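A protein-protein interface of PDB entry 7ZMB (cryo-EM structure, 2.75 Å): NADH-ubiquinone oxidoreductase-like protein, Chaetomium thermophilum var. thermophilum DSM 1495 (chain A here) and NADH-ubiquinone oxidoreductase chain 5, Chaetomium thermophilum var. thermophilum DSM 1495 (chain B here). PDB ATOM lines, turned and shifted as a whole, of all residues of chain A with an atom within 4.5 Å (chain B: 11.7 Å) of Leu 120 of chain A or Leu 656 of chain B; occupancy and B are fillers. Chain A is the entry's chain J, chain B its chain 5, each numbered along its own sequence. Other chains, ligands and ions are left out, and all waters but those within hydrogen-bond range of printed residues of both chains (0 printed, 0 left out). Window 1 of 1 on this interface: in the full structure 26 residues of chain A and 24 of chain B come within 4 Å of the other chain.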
ATOM      1  N   TYR A  69      -8.640 -23.193 -16.623  1.00  0.00           N
ATOM      2  CA  TYR A  69      -8.144 -21.939 -17.166  1.00  0.00           C
ATOM      3  C   TYR A  69      -6.994 -22.162 -18.128  1.00  0.00           C
ATOM      4  O   TYR A  69      -6.830 -21.394 -19.076  1.00  0.00           O
ATOM      5  CB  TYR A  69      -7.688 -20.994 -16.051  1.00  0.00           C
ATOM      6  CG  TYR A  69      -6.880 -19.824 -16.570  1.00  0.00           C
ATOM      7  CD1 TYR A  69      -7.423 -18.943 -17.489  1.00  0.00           C
ATOM      8  CD2 TYR A  69      -5.579 -19.608 -16.159  1.00  0.00           C
ATOM      9  CE1 TYR A  69      -6.702 -17.882 -17.982  1.00  0.00           C
ATOM     10  CE2 TYR A  69      -4.850 -18.540 -16.647  1.00  0.00           C
ATOM     11  CZ  TYR A  69      -5.422 -17.685 -17.560  1.00  0.00           C
ATOM     12  OH  TYR A  69      -4.716 -16.619 -18.052  1.00  0.00           O
ATOM     13  N   TRP A  85      -3.281 -10.908 -26.162  1.00  0.00           N
ATOM     14  CA  TRP A  85      -4.017 -10.731 -24.916  1.00  0.00           C
ATOM     15  C   TRP A  85      -5.274 -11.583 -24.866  1.00  0.00           C
ATOM     16  O   TRP A  85      -5.669 -12.038 -23.788  1.00  0.00           O
ATOM     17  CB  TRP A  85      -4.399  -9.267 -24.745  1.00  0.00           C
ATOM     18  CG  TRP A  85      -5.297  -8.783 -25.836  1.00  0.00           C
ATOM     19  CD1 TRP A  85      -4.920  -8.306 -27.053  1.00  0.00           C
ATOM     20  CD2 TRP A  85      -6.725  -8.738 -25.813  1.00  0.00           C
ATOM     21  NE1 TRP A  85      -6.023  -7.964 -27.790  1.00  0.00           N
ATOM     22  CE2 TRP A  85      -7.146  -8.222 -27.050  1.00  0.00           C
ATOM     23  CE3 TRP A  85      -7.689  -9.083 -24.866  1.00  0.00           C
ATOM     24  CZ2 TRP A  85      -8.488  -8.041 -27.365  1.00  0.00           C
ATOM     25  CZ3 TRP A  85      -9.018  -8.907 -25.179  1.00  0.00           C
ATOM     26  CH2 TRP A  85      -9.407  -8.390 -26.418  1.00  0.00           C
ATOM     27  N   ASN A  88      -5.929 -15.341 -23.176  1.00  0.00           N
ATOM     28  CA  ASN A  88      -6.154 -15.387 -21.735  1.00  0.00           C
ATOM     29  C   ASN A  88      -7.579 -14.999 -21.371  1.00  0.00           C
ATOM     30  O   ASN A  88      -8.078 -15.396 -20.313  1.00  0.00           O
ATOM     31  CB  ASN A  88      -5.152 -14.480 -21.032  1.00  0.00           C
ATOM     32  CG  ASN A  88      -3.728 -14.946 -21.218  1.00  0.00           C
ATOM     33  OD1 ASN A  88      -3.339 -16.012 -20.744  1.00  0.00           O
ATOM     34  ND2 ASN A  88      -2.945 -14.158 -21.934  1.00  0.00           N
ATOM     35  N   GLY A  89      -8.243 -14.215 -22.218  1.00  0.00           N
ATOM     36  CA  GLY A  89      -9.649 -13.930 -21.994  1.00  0.00           C
ATOM     37  C   GLY A  89     -10.526 -15.159 -22.142  1.00  0.00           C
ATOM     38  O   GLY A  89     -11.407 -15.402 -21.314  1.00  0.00           O
ATOM     39  N   GLY A  92      -9.731 -17.465 -19.216  1.00  0.00           N
ATOM     40  CA  GLY A  92     -10.402 -16.860 -18.083  1.00  0.00           C
ATOM     41  C   GLY A  92     -11.908 -16.956 -18.191  1.00  0.00           C
ATOM     42  O   GLY A  92     -12.595 -17.208 -17.200  1.00  0.00           O
ATOM     43  N   THR A 116     -14.108 -12.825 -14.391  1.00  0.00           N
ATOM     44  CA  THR A 116     -12.741 -13.279 -14.590  1.00  0.00           C
ATOM     45  C   THR A 116     -12.363 -13.354 -16.062  1.00  0.00           C
ATOM     46  O   THR A 116     -11.175 -13.443 -16.375  1.00  0.00           O
ATOM     47  CB  THR A 116     -12.555 -14.639 -13.928  1.00  0.00           C
ATOM     48  OG1 THR A 116     -11.174 -15.021 -13.977  1.00  0.00           O
ATOM     49  CG2 THR A 116     -13.370 -15.646 -14.634  1.00  0.00           C
ATOM     50  N   GLY A 117     -13.339 -13.335 -16.968  1.00  0.00           N
ATOM     51  CA  GLY A 117     -13.012 -13.216 -18.377  1.00  0.00           C
ATOM     52  C   GLY A 117     -12.497 -11.835 -18.730  1.00  0.00           C
ATOM     53  O   GLY A 117     -11.487 -11.693 -19.423  1.00  0.00           O
ATOM     54  N   VAL A 118     -13.185 -10.797 -18.246  1.00  0.00           N
ATOM     55  CA  VAL A 118     -12.770  -9.423 -18.514  1.00  0.00           C
ATOM     56  C   VAL A 118     -11.510  -9.067 -17.742  1.00  0.00           C
ATOM     57  O   VAL A 118     -10.682  -8.283 -18.227  1.00  0.00           O
ATOM     58  CB  VAL A 118     -13.920  -8.448 -18.208  1.00  0.00           C
ATOM     59  CG1 VAL A 118     -13.464  -7.015 -18.376  1.00  0.00           C
ATOM     60  CG2 VAL A 118     -15.082  -8.711 -19.146  1.00  0.00           C
ATOM     61  N   VAL A 119     -11.334  -9.613 -16.539  1.00  0.00           N
ATOM     62  CA  VAL A 119     -10.143  -9.285 -15.762  1.00  0.00           C
ATOM     63  C   VAL A 119      -8.892  -9.732 -16.499  1.00  0.00           C
ATOM     64  O   VAL A 119      -7.912  -8.986 -16.604  1.00  0.00           O
ATOM     65  CB  VAL A 119     -10.225  -9.908 -14.357  1.00  0.00           C
ATOM     66  CG1 VAL A 119      -8.846  -9.956 -13.717  1.00  0.00           C
ATOM     67  CG2 VAL A 119     -11.193  -9.130 -13.491  1.00  0.00           C
ATOM     68  N   LEU A 120      -8.914 -10.944 -17.045  1.00  0.00           N
ATOM     69  CA  LEU A 120      -7.760 -11.525 -17.709  1.00  0.00           C
ATOM     70  C   LEU A 120      -7.691 -11.163 -19.184  1.00  0.00           C
ATOM     71  O   LEU A 120      -6.811 -11.655 -19.894  1.00  0.00           O
ATOM     72  CB  LEU A 120      -7.764 -13.042 -17.526  1.00  0.00           C
ATOM     73  CG  LEU A 120      -7.949 -13.516 -16.077  1.00  0.00           C
ATOM     74  CD1 LEU A 120      -7.715 -15.005 -15.966  1.00  0.00           C
ATOM     75  CD2 LEU A 120      -7.030 -12.784 -15.135  1.00  0.00           C
ATOM     76  N   ALA A 121      -8.604 -10.334 -19.666  1.00  0.00           N
ATOM     77  CA  ALA A 121      -8.352  -9.633 -20.913  1.00  0.00           C
ATOM     78  C   ALA A 121      -7.672  -8.297 -20.656  1.00  0.00           C
ATOM     79  O   ALA A 121      -6.768  -7.901 -21.400  1.00  0.00           O
ATOM     80  CB  ALA A 121      -9.662  -9.420 -21.673  1.00  0.00           C
ATOM     81  N   THR A 122      -8.092  -7.616 -19.590  1.00  0.00           N
ATOM     82  CA  THR A 122      -7.584  -6.288 -19.279  1.00  0.00           C
ATOM     83  C   THR A 122      -6.121  -6.336 -18.866  1.00  0.00           C
ATOM     84  O   THR A 122      -5.305  -5.544 -19.348  1.00  0.00           O
ATOM     85  CB  THR A 122      -8.429  -5.671 -18.171  1.00  0.00           C
ATOM     86  OG1 THR A 122      -9.805  -5.669 -18.567  1.00  0.00           O
ATOM     87  CG2 THR A 122      -7.989  -4.262 -17.894  1.00  0.00           C
ATOM     88  N   ALA A 123      -5.768  -7.258 -17.971  1.00  0.00           N
ATOM     89  CA  ALA A 123      -4.394  -7.331 -17.494  1.00  0.00           C
ATOM     90  C   ALA A 123      -3.444  -7.878 -18.545  1.00  0.00           C
ATOM     91  O   ALA A 123      -2.230  -7.688 -18.427  1.00  0.00           O
ATOM     92  CB  ALA A 123      -4.319  -8.182 -16.229  1.00  0.00           C
ATOM     93  N   GLU A 124      -3.956  -8.547 -19.568  1.00  0.00           N
ATOM     94  CA  GLU A 124      -3.100  -9.044 -20.634  1.00  0.00           C
ATOM     95  C   GLU A 124      -2.963  -8.062 -21.783  1.00  0.00           C
ATOM     96  O   GLU A 124      -1.928  -8.047 -22.454  1.00  0.00           O
ATOM     97  CB  GLU A 124      -3.627 -10.379 -21.156  1.00  0.00           C
ATOM     98  CG  GLU A 124      -3.219 -11.602 -20.353  1.00  0.00           C
ATOM     99  CD  GLU A 124      -3.514 -11.509 -18.858  1.00  0.00           C
ATOM    100  OE1 GLU A 124      -4.668 -11.261 -18.466  1.00  0.00           O
ATOM    101  OE2 GLU A 124      -2.593 -11.759 -18.065  1.00  0.00           O
ATOM    102  N   LEU B 641       1.903 -17.423   0.883  1.00  0.00           N
ATOM    103  CA  LEU B 641       1.479 -17.169  -0.486  1.00  0.00           C
ATOM    104  C   LEU B 641       2.380 -16.163  -1.190  1.00  0.00           C
ATOM    105  O   LEU B 641       2.563 -16.254  -2.406  1.00  0.00           O
ATOM    106  CB  LEU B 641       0.026 -16.695  -0.499  1.00  0.00           C
ATOM    107  CG  LEU B 641      -1.018 -17.815  -0.485  1.00  0.00           C
ATOM    108  CD1 LEU B 641      -2.295 -17.385   0.202  1.00  0.00           C
ATOM    109  CD2 LEU B 641      -1.292 -18.277  -1.892  1.00  0.00           C
ATOM    110  N   TYR B 642       2.942 -15.199  -0.457  1.00  0.00           N
ATOM    111  CA  TYR B 642       3.873 -14.260  -1.072  1.00  0.00           C
ATOM    112  C   TYR B 642       5.179 -14.946  -1.438  1.00  0.00           C
ATOM    113  O   TYR B 642       5.797 -14.607  -2.452  1.00  0.00           O
ATOM    114  CB  TYR B 642       4.147 -13.077  -0.145  1.00  0.00           C
ATOM    115  CG  TYR B 642       3.123 -11.974  -0.205  1.00  0.00           C
ATOM    116  CD1 TYR B 642       1.805 -12.234  -0.529  1.00  0.00           C
ATOM    117  CD2 TYR B 642       3.478 -10.668   0.075  1.00  0.00           C
ATOM    118  CE1 TYR B 642       0.871 -11.218  -0.573  1.00  0.00           C
ATOM    119  CE2 TYR B 642       2.554  -9.657   0.040  1.00  0.00           C
ATOM    120  CZ  TYR B 642       1.256  -9.937  -0.288  1.00  0.00           C
ATOM    121  OH  TYR B 642       0.338  -8.926  -0.334  1.00  0.00           O
ATOM    122  N   ILE B 644       5.265 -18.200  -2.201  1.00  0.00           N
ATOM    123  CA  ILE B 644       4.859 -19.011  -3.348  1.00  0.00           C
ATOM    124  C   ILE B 644       4.862 -18.174  -4.615  1.00  0.00           C
ATOM    125  O   ILE B 644       5.386 -18.592  -5.653  1.00  0.00           O
ATOM    126  CB  ILE B 644       3.474 -19.644  -3.116  1.00  0.00           C
ATOM    127  CG1 ILE B 644       3.454 -20.537  -1.886  1.00  0.00           C
ATOM    128  CG2 ILE B 644       3.060 -20.449  -4.328  1.00  0.00           C
ATOM    129  CD1 ILE B 644       4.384 -21.677  -1.982  1.00  0.00           C
ATOM    130  N   TYR B 645       4.275 -16.978  -4.551  1.00  0.00           N
ATOM    131  CA  TYR B 645       4.175 -16.162  -5.752  1.00  0.00           C
ATOM    132  C   TYR B 645       5.548 -15.784  -6.275  1.00  0.00           C
ATOM    133  O   TYR B 645       5.774 -15.755  -7.489  1.00  0.00           O
ATOM    134  CB  TYR B 645       3.351 -14.909  -5.490  1.00  0.00           C
ATOM    135  CG  TYR B 645       3.247 -14.025  -6.707  1.00  0.00           C
ATOM    136  CD1 TYR B 645       2.568 -14.452  -7.839  1.00  0.00           C
ATOM    137  CD2 TYR B 645       3.845 -12.779  -6.738  1.00  0.00           C
ATOM    138  CE1 TYR B 645       2.472 -13.651  -8.957  1.00  0.00           C
ATOM    139  CE2 TYR B 645       3.751 -11.972  -7.845  1.00  0.00           C
ATOM    140  CZ  TYR B 645       3.065 -12.410  -8.953  1.00  0.00           C
ATOM    141  OH  TYR B 645       2.976 -11.605 -10.062  1.00  0.00           O
ATOM    142  N   LEU B 650       5.670 -17.669 -10.599  1.00  0.00           N
ATOM    143  CA  LEU B 650       4.335 -17.880 -11.129  1.00  0.00           C
ATOM    144  C   LEU B 650       3.979 -16.773 -12.112  1.00  0.00           C
ATOM    145  O   LEU B 650       4.376 -15.616 -11.952  1.00  0.00           O
ATOM    146  CB  LEU B 650       3.308 -17.912  -9.998  1.00  0.00           C
ATOM    147  CG  LEU B 650       3.392 -19.031  -8.969  1.00  0.00           C
ATOM    148  CD1 LEU B 650       2.159 -19.012  -8.085  1.00  0.00           C
ATOM    149  CD2 LEU B 650       3.546 -20.380  -9.650  1.00  0.00           C
ATOM    150  N   ASP B 651       3.241 -17.140 -13.155  1.00  0.00           N
ATOM    151  CA  ASP B 651       2.638 -16.125 -14.002  1.00  0.00           C
ATOM    152  C   ASP B 651       1.579 -15.372 -13.209  1.00  0.00           C
ATOM    153  O   ASP B 651       0.890 -15.940 -12.362  1.00  0.00           O
ATOM    154  CB  ASP B 651       2.030 -16.753 -15.254  1.00  0.00           C
ATOM    155  CG  ASP B 651       1.296 -15.743 -16.109  1.00  0.00           C
ATOM    156  OD1 ASP B 651       1.895 -14.703 -16.449  1.00  0.00           O
ATOM    157  OD2 ASP B 651       0.121 -15.991 -16.446  1.00  0.00           O
ATOM    158  N   TYR B 652       1.472 -14.072 -13.472  1.00  0.00           N
ATOM    159  CA  TYR B 652       0.590 -13.227 -12.679  1.00  0.00           C
ATOM    160  C   TYR B 652      -0.871 -13.599 -12.840  1.00  0.00           C
ATOM    161  O   TYR B 652      -1.673 -13.284 -11.956  1.00  0.00           O
ATOM    162  CB  TYR B 652       0.796 -11.759 -13.037  1.00  0.00           C
ATOM    163  CG  TYR B 652       0.462 -11.404 -14.463  1.00  0.00           C
ATOM    164  CD1 TYR B 652       1.295 -11.786 -15.509  1.00  0.00           C
ATOM    165  CD2 TYR B 652      -0.678 -10.679 -14.766  1.00  0.00           C
ATOM    166  CE1 TYR B 652       0.999 -11.461 -16.810  1.00  0.00           C
ATOM    167  CE2 TYR B 652      -0.979 -10.342 -16.060  1.00  0.00           C
ATOM    168  CZ  TYR B 652      -0.136 -10.734 -17.083  1.00  0.00           C
ATOM    169  OH  TYR B 652      -0.440 -10.408 -18.384  1.00  0.00           O
ATOM    170  N   SER B 653      -1.230 -14.271 -13.935  1.00  0.00           N
ATOM    171  CA  SER B 653      -2.626 -14.613 -14.173  1.00  0.00           C
ATOM    172  C   SER B 653      -3.166 -15.530 -13.083  1.00  0.00           C
ATOM    173  O   SER B 653      -4.324 -15.397 -12.668  1.00  0.00           O
ATOM    174  CB  SER B 653      -2.774 -15.261 -15.546  1.00  0.00           C
ATOM    175  OG  SER B 653      -4.126 -15.528 -15.839  1.00  0.00           O
ATOM    176  N   TYR B 654      -2.344 -16.468 -12.607  1.00  0.00           N
ATOM    177  CA  TYR B 654      -2.767 -17.317 -11.503  1.00  0.00           C
ATOM    178  C   TYR B 654      -3.131 -16.490 -10.283  1.00  0.00           C
ATOM    179  O   TYR B 654      -4.161 -16.732  -9.647  1.00  0.00           O
ATOM    180  CB  TYR B 654      -1.679 -18.330 -11.164  1.00  0.00           C
ATOM    181  CG  TYR B 654      -1.191 -19.110 -12.354  1.00  0.00           C
ATOM    182  CD1 TYR B 654      -1.981 -20.099 -12.925  1.00  0.00           C
ATOM    183  CD2 TYR B 654       0.049 -18.859 -12.915  1.00  0.00           C
ATOM    184  CE1 TYR B 654      -1.550 -20.817 -14.017  1.00  0.00           C
ATOM    185  CE2 TYR B 654       0.494 -19.576 -14.008  1.00  0.00           C
ATOM    186  CZ  TYR B 654      -0.310 -20.552 -14.555  1.00  0.00           C
ATOM    187  OH  TYR B 654       0.128 -21.267 -15.645  1.00  0.00           O
ATOM    188  N   LEU B 655      -2.312 -15.493  -9.958  1.00  0.00           N
ATOM    189  CA  LEU B 655      -2.605 -14.638  -8.814  1.00  0.00           C
ATOM    190  C   LEU B 655      -3.928 -13.908  -8.993  1.00  0.00           C
ATOM    191  O   LEU B 655      -4.747 -13.856  -8.070  1.00  0.00           O
ATOM    192  CB  LEU B 655      -1.456 -13.659  -8.604  1.00  0.00           C
ATOM    193  CG  LEU B 655      -1.504 -12.730  -7.402  1.00  0.00           C
ATOM    194  CD1 LEU B 655      -0.104 -12.567  -6.940  1.00  0.00           C
ATOM    195  CD2 LEU B 655      -2.050 -11.387  -7.822  1.00  0.00           C
ATOM    196  N   LEU B 656      -4.161 -13.342 -10.176  1.00  0.00           N
ATOM    197  CA  LEU B 656      -5.452 -12.713 -10.437  1.00  0.00           C
ATOM    198  C   LEU B 656      -6.586 -13.720 -10.307  1.00  0.00           C
ATOM    199  O   LEU B 656      -7.612 -13.436  -9.681  1.00  0.00           O
ATOM    200  CB  LEU B 656      -5.464 -12.083 -11.823  1.00  0.00           C
ATOM    201  CG  LEU B 656      -4.835 -10.705 -11.963  1.00  0.00           C
ATOM    202  CD1 LEU B 656      -4.756 -10.340 -13.423  1.00  0.00           C
ATOM    203  CD2 LEU B 656      -5.637  -9.669 -11.213  1.00  0.00           C
ATOM    204  N   LEU B 657      -6.407 -14.910 -10.870  1.00  0.00           N
ATOM    205  CA  LEU B 657      -7.451 -15.920 -10.803  1.00  0.00           C
ATOM    206  C   LEU B 657      -7.656 -16.407  -9.378  1.00  0.00           C
ATOM    207  O   LEU B 657      -8.790 -16.643  -8.953  1.00  0.00           O
ATOM    208  CB  LEU B 657      -7.110 -17.077 -11.735  1.00  0.00           C
ATOM    209  CG  LEU B 657      -8.221 -18.104 -11.839  1.00  0.00           C
ATOM    210  CD1 LEU B 657      -9.454 -17.383 -12.308  1.00  0.00           C
ATOM    211  CD2 LEU B 657      -7.833 -19.181 -12.828  1.00  0.00           C
ATOM    212  N   ILE B 658      -6.568 -16.558  -8.621  1.00  0.00           N
ATOM    213  CA  ILE B 658      -6.680 -16.939  -7.218  1.00  0.00           C
ATOM    214  C   ILE B 658      -7.486 -15.902  -6.444  1.00  0.00           C
ATOM    215  O   ILE B 658      -8.326 -16.251  -5.609  1.00  0.00           O
ATOM    216  CB  ILE B 658      -5.279 -17.155  -6.614  1.00  0.00           C
ATOM    217  CG1 ILE B 658      -4.661 -18.445  -7.149  1.00  0.00           C
ATOM    218  CG2 ILE B 658      -5.333 -17.220  -5.105  1.00  0.00           C
ATOM    219  CD1 ILE B 658      -3.317 -18.771  -6.550  1.00  0.00           C
ATOM    220  N   ILE B 659      -7.258 -14.615  -6.718  1.00  0.00           N
ATOM    221  CA  ILE B 659      -7.978 -13.553  -6.013  1.00  0.00           C
ATOM    222  C   ILE B 659      -9.448 -13.535  -6.411  1.00  0.00           C
ATOM    223  O   ILE B 659     -10.335 -13.448  -5.555  1.00  0.00           O
ATOM    224  CB  ILE B 659      -7.310 -12.191  -6.266  1.00  0.00           C
ATOM    225  CG1 ILE B 659      -6.038 -12.073  -5.443  1.00  0.00           C
ATOM    226  CG2 ILE B 659      -8.254 -11.050  -5.936  1.00  0.00           C
ATOM    227  CD1 ILE B 659      -5.056 -11.134  -6.028  1.00  0.00           C
ATOM    228  N   ILE B 660      -9.732 -13.605  -7.709  1.00  0.00           N
ATOM    229  CA  ILE B 660     -11.120 -13.711  -8.152  1.00  0.00           C
ATOM    230  C   ILE B 660     -11.769 -14.946  -7.551  1.00  0.00           C
ATOM    231  O   ILE B 660     -12.915 -14.906  -7.090  1.00  0.00           O
ATOM    232  CB  ILE B 660     -11.196 -13.732  -9.689  1.00  0.00           C
ATOM    233  CG1 ILE B 660     -10.616 -12.455 -10.279  1.00  0.00           C
ATOM    234  CG2 ILE B 660     -12.599 -13.966 -10.148  1.00  0.00           C
ATOM    235  CD1 ILE B 660     -11.156 -11.220  -9.648  1.00  0.00           C
ATOM    236  N   LEU B 661     -11.043 -16.061  -7.538  1.00  0.00           N
ATOM    237  CA  LEU B 661     -11.598 -17.285  -6.983  1.00  0.00           C
ATOM    238  C   LEU B 661     -11.864 -17.130  -5.490  1.00  0.00           C
ATOM    239  O   LEU B 661     -12.911 -17.555  -4.997  1.00  0.00           O
ATOM    240  CB  LEU B 661     -10.654 -18.449  -7.280  1.00  0.00           C
ATOM    241  CG  LEU B 661     -11.012 -19.871  -6.876  1.00  0.00           C
ATOM    242  CD1 LEU B 661     -12.270 -20.314  -7.601  1.00  0.00           C
ATOM    243  CD2 LEU B 661      -9.866 -20.772  -7.251  1.00  0.00           C
ATOM    244  N   LEU B 662     -10.948 -16.490  -4.759  1.00  0.00           N
ATOM    245  CA  LEU B 662     -11.187 -16.254  -3.338  1.00  0.00           C
ATOM    246  C   LEU B 662     -12.326 -15.269  -3.121  1.00  0.00           C
ATOM    247  O   LEU B 662     -13.211 -15.510  -2.294  1.00  0.00           O
ATOM    248  CB  LEU B 662      -9.924 -15.749  -2.649  1.00  0.00           C
ATOM    249  CG  LEU B 662      -8.737 -16.697  -2.483  1.00  0.00           C
ATOM    250  CD1 LEU B 662      -7.451 -15.910  -2.561  1.00  0.00           C
ATOM    251  CD2 LEU B 662      -8.819 -17.447  -1.178  1.00  0.00           C
ATOM    252  N   LEU B 663     -12.320 -14.155  -3.849  1.00  0.00           N
ATOM    253  CA  LEU B 663     -13.393 -13.176  -3.709  1.00  0.00           C
ATOM    254  C   LEU B 663     -14.742 -13.800  -4.021  1.00  0.00           C
ATOM    255  O   LEU B 663     -15.755 -13.453  -3.406  1.00  0.00           O
ATOM    256  CB  LEU B 663     -13.140 -11.981  -4.628  1.00  0.00           C
ATOM    257  CG  LEU B 663     -12.403 -10.772  -4.054  1.00  0.00           C
ATOM    258  CD1 LEU B 663     -13.310  -9.993  -3.131  1.00  0.00           C
ATOM    259  CD2 LEU B 663     -11.140 -11.192  -3.328  1.00  0.00           C
ATOM    260  N   LEU B 664     -14.769 -14.734  -4.960  1.00  0.00           N
ATOM    261  CA  LEU B 664     -16.040 -15.278  -5.409  1.00  0.00           C
ATOM    262  C   LEU B 664     -16.321 -16.646  -4.799  1.00  0.00           C
ATOM    263  O   LEU B 664     -17.328 -17.277  -5.124  1.00  0.00           O
ATOM    264  CB  LEU B 664     -16.051 -15.309  -6.931  1.00  0.00           C
ATOM    265  CG  LEU B 664     -15.965 -13.857  -7.414  1.00  0.00           C
ATOM    266  CD1 LEU B 664     -15.808 -13.729  -8.909  1.00  0.00           C
ATOM    267  CD2 LEU B 664     -17.188 -13.077  -6.941  1.00  0.00           C
ATOM    268  N   LEU B 665     -15.446 -17.122  -3.915  1.00  0.00           N
ATOM    269  CA  LEU B 665     -15.874 -18.144  -2.967  1.00  0.00           C
ATOM    270  C   LEU B 665     -16.219 -17.500  -1.635  1.00  0.00           C
ATOM    271  O   LEU B 665     -16.984 -18.057  -0.841  1.00  0.00           O
ATOM    272  CB  LEU B 665     -14.803 -19.224  -2.801  1.00  0.00           C
ATOM    273  CG  LEU B 665     -13.401 -18.924  -2.264  1.00  0.00           C
ATOM    274  CD1 LEU B 665     -13.365 -18.895  -0.741  1.00  0.00           C
ATOM    275  CD2 LEU B 665     -12.398 -19.930  -2.799  1.00  0.00           C
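The side-chain hydroxyl of Tyr 69 of chain A is in hydrogen-bond range of the side-chain amide oxygen of Asn 88 of chain A, at 3.1 Å. N of Ser 653 of chain B lies close to OD2 of Asp 651 of chain B (3.3 Å). OE1 of Glu 124 of chain A sits close to O of Leu 120 of chain A.
Leu 120 of chain A touches just these residues of chain B: Ser 653 (3.6 Å) and Leu 656 (3.7 Å). Of the printed residues of chain A, Leu 656 of chain B touches Leu 120 and Ala 123. Asn 88 of chain A touches none of the printed residues of chain B. No residue of chain B comes within 4 Å of Gly 89 of chain A. Gly 92 of chain A touches none of the printed residues of chain B. Thr 116 of chain A touches just these residues of chain B: Leu 657 and Ile 660. No residue of chain B comes within 4 Å of Gly 117 of chain A. No residue of chain B comes within 4 Å of Val 119 of chain A. No residue of chain B comes within 4 Å of Ala 121 of chain A. No residue of chain B comes within 4 Å of Thr 122 of chain A. Ala 123 of chain A touches just these residues of chain B: Tyr 652 (3.3 Å) and Leu 656 (3.6 Å). Glu 124 of chain A touches just one residue of chain B: Tyr 652. Printed residues of chain A within 4 Å of Ser 653 of chain B: Tyr 69 (2.5 Å) and Leu 120 (3.6 Å). Printed residues of chain A within 4 Å of Ile 660 of chain B: Thr 116. Of the printed residues of chain A, Tyr 652 of chain B touches Ala 123 and Glu 124. Of the printed residues of chain A, Leu 657 of chain B touches Tyr 69 (3.7 Å) and Thr 116 (3.4 Å).
Tyr 69 of chain A touches Leu 657 of chain B (CB to CD2, 3.7 Å). Thr 116 of chain A touches Leu 657 of chain B (OG1 to CD1, 3.4 Å). Ile 660 of chain B touches Thr 116 of chain A (CG2 to CB, 3.8 Å). Ser 653 of chain B touches Leu 120 of chain A (OG to CD1, 3.6 Å). CB of Leu 656 of chain B touches CD2 of Leu 120 of chain A, 3.7 Å away. CB of Ala 123 of chain A touches CD1 of Leu 656 of chain B, 3.6 Å away.
Hydrophobic or aromatic side chains of chain B that line the printed part of chain A: Tyr 652, Leu 656, Leu 657 and Ile 660. Along chain B the printed residues that touch a printed residue of chain A span positions 652 to 660. Of the 14 printed residues of chain A, 5 touch a printed residue of chain B. Among the printed residues, 9 pairs touch across the chains.
O of Ala 123 of chain A is in hydrogen-bond range of OH of Tyr 652 of chain B (3.3 Å). OH of Tyr 652 of chain B lies within hydrogen-bond range of OE2 of Glu 124 of chain A, at 2.6 Å. The side-chain hydroxyl (OH) of Tyr 69 of chain A is in hydrogen-bond range of the side-chain hydroxyl (OG) of Ser 653 of chain B (2.5 Å).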
